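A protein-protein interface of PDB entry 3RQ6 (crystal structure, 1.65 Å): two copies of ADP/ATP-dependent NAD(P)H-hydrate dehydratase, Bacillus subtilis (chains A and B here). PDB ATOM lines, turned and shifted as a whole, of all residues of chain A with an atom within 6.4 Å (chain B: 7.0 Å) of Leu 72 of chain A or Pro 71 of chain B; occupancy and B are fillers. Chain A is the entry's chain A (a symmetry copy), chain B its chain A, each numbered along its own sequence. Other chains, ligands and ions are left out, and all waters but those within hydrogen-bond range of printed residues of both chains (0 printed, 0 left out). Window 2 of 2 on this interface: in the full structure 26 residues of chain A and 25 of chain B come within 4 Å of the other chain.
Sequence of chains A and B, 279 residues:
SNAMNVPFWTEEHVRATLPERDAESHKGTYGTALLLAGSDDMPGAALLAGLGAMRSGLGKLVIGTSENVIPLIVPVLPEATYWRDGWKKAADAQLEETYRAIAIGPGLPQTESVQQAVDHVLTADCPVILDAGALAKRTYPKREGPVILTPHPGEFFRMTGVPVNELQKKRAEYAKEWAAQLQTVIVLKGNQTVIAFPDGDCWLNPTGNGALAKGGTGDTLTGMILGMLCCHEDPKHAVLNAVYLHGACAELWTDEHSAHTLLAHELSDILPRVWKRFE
The side-chain carboxylate (OE2) of Glu 67 of chain B is in salt-bridge range of the guanidinium group (NH1) of Arg 84 of chain B (2.8 Å).
The guanidinium group (NH2) of Arg 84 of chain B sits at hydrogen-bond distance from the backbone carbonyl oxygen (O) of Asp 40 of chain A (3.1 Å).
Among the printed residues, pairs that only touch across the chains: Pro 43 of chain A with Val 74 of chain B (3.6 Å), Gly 44 of chain A with Val 74 of chain B (3.99 Å), Leu 47 of chain A with Pro 75 of chain B (3.9 Å), Leu 72 of chain A with Pro 71 of chain B (3.5 Å), Leu 72 of chain A with Val 74 of chain B (3.9 Å), Leu 72 of chain A with Pro 75 of chain B (3.7 Å) and Val 76 of chain A with Pro 75 of chain B (3.5 Å).
Leu 72 of chain A touches Pro 71 of chain B, but with the chains exchanged Pro 71 of chain A does not touch Leu 72 of chain B (8.6 Å).
Leu 72 of chain A touches Val 74 of chain B, but with the chains exchanged Val 74 of chain A does not touch Leu 72 of chain B (11.9 Å).
Leu 72 of chain A touches Pro 75 of chain B, but with the chains exchanged Pro 75 of chain A does not touch Leu 72 of chain B (9.4 Å).
Val 76 of chain A touches Pro 75 of chain B, but with the chains exchanged Pro 75 of chain A does not touch Val 76 of chain B (8.3 Å).
Positions printed for both chains: 68, 69, 70, 71, 72, 73, 74, 75 and 76.
Of the printed residues of chain A, Arg 84 of chain B touches Asp 40 (3.1 Å).
Printed residues of chain A within 4 Å of Val 74 of chain B: Pro 43 (3.6 Å), Gly 44 (3.99 Å) and Leu 72 (3.9 Å).
Of the printed residues of chain B, Pro 43 of chain A touches Val 74 (3.6 Å).
Of the printed residues of chain B, Leu 47 of chain A touches Pro 75.
Glu 67 of chain B touches none of the printed residues of chain A.
The nearest residue of chain A that does not touch Pro 71 of chain B is Asn 68 of chain A (6.0 Å).
The nearest printed residue of chain B that does not touch Leu 47 of chain A is Val 74 of chain B (4.1 Å).
Hydrophobic or aromatic side chains of chain B that line the printed part of chain A: Pro 71, Val 74 and Pro 75.
Printed residues of chain A that touch a printed residue of chain B: Asp 40, Pro 43, Gly 44, Leu 47, Leu 72 and Val 76.
Hydrophobic or aromatic side chains of chain A that line the printed part of chain B: Pro 43, Leu 47, Leu 72 and Val 76.
Along chain A the printed residues that touch a printed residue of chain B span positions 40 to 76.
Among the printed residues, 8 pairs touch across the chains.
Among the printed residues, no Asp or Glu carboxylate lies within 4 Å of a Lys or Arg side-chain nitrogen of the other chain.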
ATOM      1  N   ASP A  40      -5.471  13.546  10.535  1.00  0.00           N
ATOM      2  CA  ASP A  40      -5.304  14.643  11.448  1.00  0.00           C
ATOM      3  C   ASP A  40      -6.153  14.600  12.733  1.00  0.00           C
ATOM      4  O   ASP A  40      -5.635  14.889  13.740  1.00  0.00           O
ATOM      5  CB  ASP A  40      -5.346  16.016  10.716  1.00  0.00           C
ATOM      6  CG  ASP A  40      -4.170  16.232   9.748  1.00  0.00           C
ATOM      7  OD1 ASP A  40      -3.206  15.480   9.673  1.00  0.00           O
ATOM      8  OD2 ASP A  40      -4.206  17.210   9.010  1.00  0.00           O
ATOM      9  N   PRO A  43      -5.294  10.613  14.733  1.00  0.00           N
ATOM     10  CA  PRO A  43      -3.908  10.235  14.485  1.00  0.00           C
ATOM     11  C   PRO A  43      -3.449   8.968  15.206  1.00  0.00           C
ATOM     12  O   PRO A  43      -2.561   8.220  14.761  1.00  0.00           O
ATOM     13  CB  PRO A  43      -3.115  11.409  15.062  1.00  0.00           C
ATOM     14  CG  PRO A  43      -4.045  12.043  16.078  1.00  0.00           C
ATOM     15  CD  PRO A  43      -5.421  11.836  15.523  1.00  0.00           C
ATOM     16  N   GLY A  44      -4.047   8.747  16.369  1.00  0.00           N
ATOM     17  CA  GLY A  44      -3.567   7.711  17.266  1.00  0.00           C
ATOM     18  C   GLY A  44      -3.666   6.314  16.712  1.00  0.00           C
ATOM     19  O   GLY A  44      -2.827   5.424  17.037  1.00  0.00           O
ATOM     20  N   LEU A  47      -0.355   5.018  15.388  1.00  0.00           N
ATOM     21  CA  LEU A  47       0.577   4.589  16.371  1.00  0.00           C
ATOM     22  C   LEU A  47       0.169   3.226  16.916  1.00  0.00           C
ATOM     23  O   LEU A  47       0.999   2.310  17.075  1.00  0.00           O
ATOM     24  CB  LEU A  47       0.705   5.622  17.503  1.00  0.00           C
ATOM     25  CG  LEU A  47       1.638   5.209  18.631  1.00  0.00           C
ATOM     26  CD1 LEU A  47       3.053   4.704  18.102  1.00  0.00           C
ATOM     27  CD2 LEU A  47       1.793   6.418  19.607  1.00  0.00           C
ATOM     28  N   ASN A  68       1.319  15.374   9.277  1.00  0.00           N
ATOM     29  CA  ASN A  68       1.275  15.830  10.650  1.00  0.00           C
ATOM     30  C   ASN A  68       1.216  14.734  11.699  1.00  0.00           C
ATOM     31  O   ASN A  68       1.389  15.006  12.872  1.00  0.00           O
ATOM     32  CB  ASN A  68       0.150  16.819  10.850  1.00  0.00           C
ATOM     33  CG  ASN A  68       0.353  18.063  10.004  1.00  0.00           C
ATOM     34  OD1 ASN A  68       1.506  18.427   9.658  1.00  0.00           O
ATOM     35  ND2 ASN A  68      -0.735  18.705   9.639  1.00  0.00           N
ATOM     36  N   VAL A  69       0.934  13.522  11.248  1.00  0.00           N
ATOM     37  CA  VAL A  69       0.884  12.369  12.151  1.00  0.00           C
ATOM     38  C   VAL A  69       2.270  11.761  12.405  1.00  0.00           C
ATOM     39  O   VAL A  69       2.552  11.150  13.469  1.00  0.00           O
ATOM     40  CB  VAL A  69      -0.166  11.352  11.655  1.00  0.00           C
ATOM     41  CG1 VAL A  69      -0.227  10.085  12.600  1.00  0.00           C
ATOM     42  CG2 VAL A  69      -1.529  12.042  11.533  1.00  0.00           C
ATOM     43  N   ILE A  70       3.107  11.767  11.380  1.00  0.00           N
ATOM     44  CA  ILE A  70       4.464  11.238  11.458  1.00  0.00           C
ATOM     45  C   ILE A  70       5.185  11.611  12.763  1.00  0.00           C
ATOM     46  O   ILE A  70       5.688  10.730  13.428  1.00  0.00           O
ATOM     47  CB  ILE A  70       5.318  11.589  10.233  1.00  0.00           C
ATOM     48  CG1 ILE A  70       4.735  10.955   8.975  1.00  0.00           C
ATOM     49  CG2 ILE A  70       6.806  11.146  10.399  1.00  0.00           C
ATOM     50  CD1 ILE A  70       5.430  11.393   7.652  1.00  0.00           C
ATOM     51  N   PRO A  71       5.248  12.864  13.111  1.00  0.00           N
ATOM     52  CA  PRO A  71       6.024  13.238  14.328  1.00  0.00           C
ATOM     53  C   PRO A  71       5.460  12.638  15.651  1.00  0.00           C
ATOM     54  O   PRO A  71       6.173  12.578  16.656  1.00  0.00           O
ATOM     55  CB  PRO A  71       5.999  14.739  14.311  1.00  0.00           C
ATOM     56  CG  PRO A  71       4.834  15.103  13.476  1.00  0.00           C
ATOM     57  CD  PRO A  71       4.776  14.080  12.394  1.00  0.00           C
ATOM     58  N   LEU A  72       4.186  12.203  15.626  1.00  0.00           N
ATOM     59  CA  LEU A  72       3.522  11.651  16.803  1.00  0.00           C
ATOM     60  C   LEU A  72       3.867  10.217  17.002  1.00  0.00           C
ATOM     61  O   LEU A  72       3.630   9.653  18.105  1.00  0.00           O
ATOM     62  CB  LEU A  72       1.993  11.886  16.674  1.00  0.00           C
ATOM     63  CG  LEU A  72       1.582  13.283  16.240  1.00  0.00           C
ATOM     64  CD1 LEU A  72       0.017  13.374  16.225  1.00  0.00           C
ATOM     65  CD2 LEU A  72       2.295  14.343  17.138  1.00  0.00           C
ATOM     66  N   ILE A  73       4.370   9.551  15.941  1.00  0.00           N
ATOM     67  CA  ILE A  73       4.714   8.159  15.994  1.00  0.00           C
ATOM     68  C   ILE A  73       6.175   7.914  16.353  1.00  0.00           C
ATOM     69  O   ILE A  73       6.493   7.030  17.166  1.00  0.00           O
ATOM     70  CB  ILE A  73       4.390   7.427  14.622  1.00  0.00           C
ATOM     71  CG1 ILE A  73       2.892   7.507  14.343  1.00  0.00           C
ATOM     72  CG2 ILE A  73       4.876   5.959  14.677  1.00  0.00           C
ATOM     73  CD1 ILE A  73       2.552   7.206  12.861  1.00  0.00           C
ATOM     74  N   VAL A  74       7.052   8.677  15.742  1.00  0.00           N
ATOM     75  CA  VAL A  74       8.494   8.480  15.822  1.00  0.00           C
ATOM     76  C   VAL A  74       9.066   8.274  17.225  1.00  0.00           C
ATOM     77  O   VAL A  74       9.818   7.338  17.443  1.00  0.00           O
ATOM     78  CB  VAL A  74       9.225   9.621  15.071  1.00  0.00           C
ATOM     79  CG1 VAL A  74      10.757   9.433  15.208  1.00  0.00           C
ATOM     80  CG2 VAL A  74       8.789   9.634  13.590  1.00  0.00           C
ATOM     81  N   PRO A  75       8.715   9.109  18.224  1.00  0.00           N
ATOM     82  CA  PRO A  75       9.364   8.943  19.546  1.00  0.00           C
ATOM     83  C   PRO A  75       8.991   7.643  20.216  1.00  0.00           C
ATOM     84  O   PRO A  75       9.759   7.158  21.043  1.00  0.00           O
ATOM     85  CB  PRO A  75       8.835  10.121  20.377  1.00  0.00           C
ATOM     86  CG  PRO A  75       8.215  11.083  19.368  1.00  0.00           C
ATOM     87  CD  PRO A  75       7.881  10.322  18.132  1.00  0.00           C
ATOM     88  N   VAL A  76       7.841   7.068  19.834  1.00  0.00           N
ATOM     89  CA  VAL A  76       7.350   5.826  20.437  1.00  0.00           C
ATOM     90  C   VAL A  76       7.784   4.567  19.631  1.00  0.00           C
ATOM     91  O   VAL A  76       8.117   3.515  20.247  1.00  0.00           O
ATOM     92  CB  VAL A  76       5.807   5.865  20.629  1.00  0.00           C
ATOM     93  CG1 VAL A  76       5.276   4.590  21.245  1.00  0.00           C
ATOM     94  CG2 VAL A  76       5.369   7.112  21.486  1.00  0.00           C
ATOM     95  N   THR B  65      -9.596  19.802  22.644  1.00  0.00           N
ATOM     96  CA  THR B  65      -8.500  20.659  23.098  1.00  0.00           C
ATOM     97  C   THR B  65      -8.065  21.561  21.971  1.00  0.00           C
ATOM     98  O   THR B  65      -8.348  21.356  20.806  1.00  0.00           O
ATOM     99  CB  THR B  65      -7.369  19.850  23.667  1.00  0.00           C
ATOM    100  OG1 THR B  65      -6.444  20.685  24.404  1.00  0.00           O
ATOM    101  CG2 THR B  65      -6.626  19.063  22.583  1.00  0.00           C
ATOM    102  N   SER B  66      -7.258  22.539  22.345  1.00  0.00           N
ATOM    103  CA  SER B  66      -6.641  23.407  21.402  1.00  0.00           C
ATOM    104  C   SER B  66      -5.809  22.637  20.379  1.00  0.00           C
ATOM    105  O   SER B  66      -5.134  21.638  20.674  1.00  0.00           O
ATOM    106  CB  SER B  66      -5.784  24.477  22.130  1.00  0.00           C
ATOM    107  OG  SER B  66      -6.612  25.328  22.920  1.00  0.00           O
ATOM    108  N   GLU B  67      -5.803  23.115  19.154  1.00  0.00           N
ATOM    109  CA  GLU B  67      -5.104  22.479  18.105  1.00  0.00           C
ATOM    110  C   GLU B  67      -3.646  22.137  18.415  1.00  0.00           C
ATOM    111  O   GLU B  67      -3.207  21.074  18.080  1.00  0.00           O
ATOM    112  CB  GLU B  67      -5.158  23.398  16.872  1.00  0.00           C
ATOM    113  CG  GLU B  67      -4.379  22.959  15.766  1.00  0.00           C
ATOM    114  CD  GLU B  67      -4.926  23.601  14.464  1.00  0.00           C
ATOM    115  OE1 GLU B  67      -5.180  24.811  14.460  1.00  0.00           O
ATOM    116  OE2 GLU B  67      -5.134  22.866  13.503  1.00  0.00           O
ATOM    117  N   ASN B  68      -2.903  23.049  19.050  1.00  0.00           N
ATOM    118  CA  ASN B  68      -1.508  22.834  19.375  1.00  0.00           C
ATOM    119  C   ASN B  68      -1.247  21.863  20.512  1.00  0.00           C
ATOM    120  O   ASN B  68      -0.117  21.458  20.717  1.00  0.00           O
ATOM    121  CB  ASN B  68      -0.809  24.149  19.625  1.00  0.00           C
ATOM    122  CG  ASN B  68      -0.818  25.024  18.385  1.00  0.00           C
ATOM    123  OD1 ASN B  68      -0.887  24.515  17.237  1.00  0.00           O
ATOM    124  ND2 ASN B  68      -0.779  26.323  18.586  1.00  0.00           N
ATOM    125  N   VAL B  69      -2.299  21.544  21.248  1.00  0.00           N
ATOM    126  CA  VAL B  69      -2.189  20.588  22.354  1.00  0.00           C
ATOM    127  C   VAL B  69      -2.297  19.131  21.883  1.00  0.00           C
ATOM    128  O   VAL B  69      -1.748  18.183  22.502  1.00  0.00           O
ATOM    129  CB  VAL B  69      -3.182  20.960  23.477  1.00  0.00           C
ATOM    130  CG1 VAL B  69      -3.100  19.931  24.676  1.00  0.00           C
ATOM    131  CG2 VAL B  69      -2.918  22.398  23.937  1.00  0.00           C
ATOM    132  N   ILE B  70      -3.134  18.900  20.884  1.00  0.00           N
ATOM    133  CA  ILE B  70      -3.344  17.575  20.314  1.00  0.00           C
ATOM    134  C   ILE B  70      -2.042  16.777  20.139  1.00  0.00           C
ATOM    135  O   ILE B  70      -1.972  15.660  20.605  1.00  0.00           O
ATOM    136  CB  ILE B  70      -4.156  17.603  19.012  1.00  0.00           C
ATOM    137  CG1 ILE B  70      -5.563  18.133  19.270  1.00  0.00           C
ATOM    138  CG2 ILE B  70      -4.244  16.198  18.336  1.00  0.00           C
ATOM    139  CD1 ILE B  70      -6.409  18.362  17.983  1.00  0.00           C
ATOM    140  N   PRO B  71      -1.056  17.318  19.483  1.00  0.00           N
ATOM    141  CA  PRO B  71       0.174  16.513  19.235  1.00  0.00           C
ATOM    142  C   PRO B  71       0.932  16.095  20.530  1.00  0.00           C
ATOM    143  O   PRO B  71       1.745  15.166  20.499  1.00  0.00           O
ATOM    144  CB  PRO B  71       0.993  17.395  18.338  1.00  0.00           C
ATOM    145  CG  PRO B  71       0.485  18.766  18.564  1.00  0.00           C
ATOM    146  CD  PRO B  71      -0.984  18.624  18.773  1.00  0.00           C
ATOM    147  N   LEU B  72       0.653  16.789  21.649  1.00  0.00           N
ATOM    148  CA  LEU B  72       1.315  16.525  22.923  1.00  0.00           C
ATOM    149  C   LEU B  72       0.689  15.379  23.637  1.00  0.00           C
ATOM    150  O   LEU B  72       1.289  14.823  24.597  1.00  0.00           O
ATOM    151  CB  LEU B  72       1.318  17.827  23.768  1.00  0.00           C
ATOM    152  CG  LEU B  72       1.728  19.086  23.023  1.00  0.00           C
ATOM    153  CD1 LEU B  72       1.744  20.291  24.028  1.00  0.00           C
ATOM    154  CD2 LEU B  72       3.073  18.837  22.271  1.00  0.00           C
ATOM    155  N   ILE B  73      -0.556  15.022  23.257  1.00  0.00           N
ATOM    156  CA  ILE B  73      -1.281  13.956  23.886  1.00  0.00           C
ATOM    157  C   ILE B  73      -1.098  12.612  23.189  1.00  0.00           C
ATOM    158  O   ILE B  73      -0.910  11.574  23.844  1.00  0.00           O
ATOM    159  CB  ILE B  73      -2.833  14.282  23.979  1.00  0.00           C
ATOM    160  CG1 ILE B  73      -3.041  15.528  24.834  1.00  0.00           C
ATOM    161  CG2 ILE B  73      -3.596  13.067  24.558  1.00  0.00           C
ATOM    162  CD1 ILE B  73      -4.445  16.154  24.633  1.00  0.00           C
ATOM    163  N   VAL B  74      -1.171  12.631  21.877  1.00  0.00           N
ATOM    164  CA  VAL B  74      -1.194  11.433  21.048  1.00  0.00           C
ATOM    165  C   VAL B  74      -0.134  10.377  21.366  1.00  0.00           C
ATOM    166  O   VAL B  74      -0.463   9.211  21.510  1.00  0.00           O
ATOM    167  CB  VAL B  74      -1.174  11.826  19.550  1.00  0.00           C
ATOM    168  CG1 VAL B  74      -1.144  10.546  18.678  1.00  0.00           C
ATOM    169  CG2 VAL B  74      -2.404  12.701  19.225  1.00  0.00           C
ATOM    170  N   PRO B  75       1.155  10.742  21.515  1.00  0.00           N
ATOM    171  CA  PRO B  75       2.171   9.683  21.722  1.00  0.00           C
ATOM    172  C   PRO B  75       2.001   8.966  23.040  1.00  0.00           C
ATOM    173  O   PRO B  75       2.429   7.820  23.153  1.00  0.00           O
ATOM    174  CB  PRO B  75       3.509  10.436  21.715  1.00  0.00           C
ATOM    175  CG  PRO B  75       3.197  11.813  21.137  1.00  0.00           C
ATOM    176  CD  PRO B  75       1.741  12.080  21.311  1.00  0.00           C
ATOM    177  N   VAL B  76       1.348   9.621  24.011  1.00  0.00           N
ATOM    178  CA  VAL B  76       1.152   9.049  25.345  1.00  0.00           C
ATOM    179  C   VAL B  76      -0.212   8.309  25.476  1.00  0.00           C
ATOM    180  O   VAL B  76      -0.279   7.236  26.140  1.00  0.00           O
ATOM    181  CB  VAL B  76       1.312  10.130  26.451  1.00  0.00           C
ATOM    182  CG1 VAL B  76       1.108   9.563  27.838  1.00  0.00           C
ATOM    183  CG2 VAL B  76       2.712  10.846  26.351  1.00  0.00           C
ATOM    184  N   TYR B  82     -10.137  13.274  18.786  1.00  0.00           N
ATOM    185  CA  TYR B  82     -10.133  14.724  19.017  1.00  0.00           C
ATOM    186  C   TYR B  82     -11.290  15.450  18.356  1.00  0.00           C
ATOM    187  O   TYR B  82     -11.751  15.050  17.282  1.00  0.00           O
ATOM    188  CB  TYR B  82      -8.818  15.374  18.480  1.00  0.00           C
ATOM    189  CG  TYR B  82      -7.707  14.752  19.245  1.00  0.00           C
ATOM    190  CD1 TYR B  82      -7.343  15.238  20.462  1.00  0.00           C
ATOM    191  CD2 TYR B  82      -7.079  13.635  18.760  1.00  0.00           C
ATOM    192  CE1 TYR B  82      -6.419  14.582  21.253  1.00  0.00           C
ATOM    193  CE2 TYR B  82      -6.165  12.932  19.529  1.00  0.00           C
ATOM    194  CZ  TYR B  82      -5.758  13.449  20.757  1.00  0.00           C
ATOM    195  OH  TYR B  82      -4.886  12.749  21.594  1.00  0.00           O
ATOM    196  N   ARG B  84     -11.164  19.105  17.275  1.00  0.00           N
ATOM    197  CA  ARG B  84     -10.160  20.155  17.169  1.00  0.00           C
ATOM    198  C   ARG B  84     -10.697  21.499  17.632  1.00  0.00           C
ATOM    199  O   ARG B  84     -11.724  21.968  17.137  1.00  0.00           O
ATOM    200  CB  ARG B  84      -9.669  20.240  15.736  1.00  0.00           C
ATOM    201  CG  ARG B  84      -8.508  21.099  15.467  1.00  0.00           C
ATOM    202  CD  ARG B  84      -8.013  20.894  13.940  1.00  0.00           C
ATOM    203  NE  ARG B  84      -7.432  19.553  13.864  1.00  0.00           N
ATOM    204  CZ  ARG B  84      -6.162  19.228  14.101  1.00  0.00           C
ATOM    205  NH1 ARG B  84      -5.229  20.166  14.227  1.00  0.00           N
ATOM    206  NH2 ARG B  84      -5.805  17.934  14.193  1.00  0.00           N
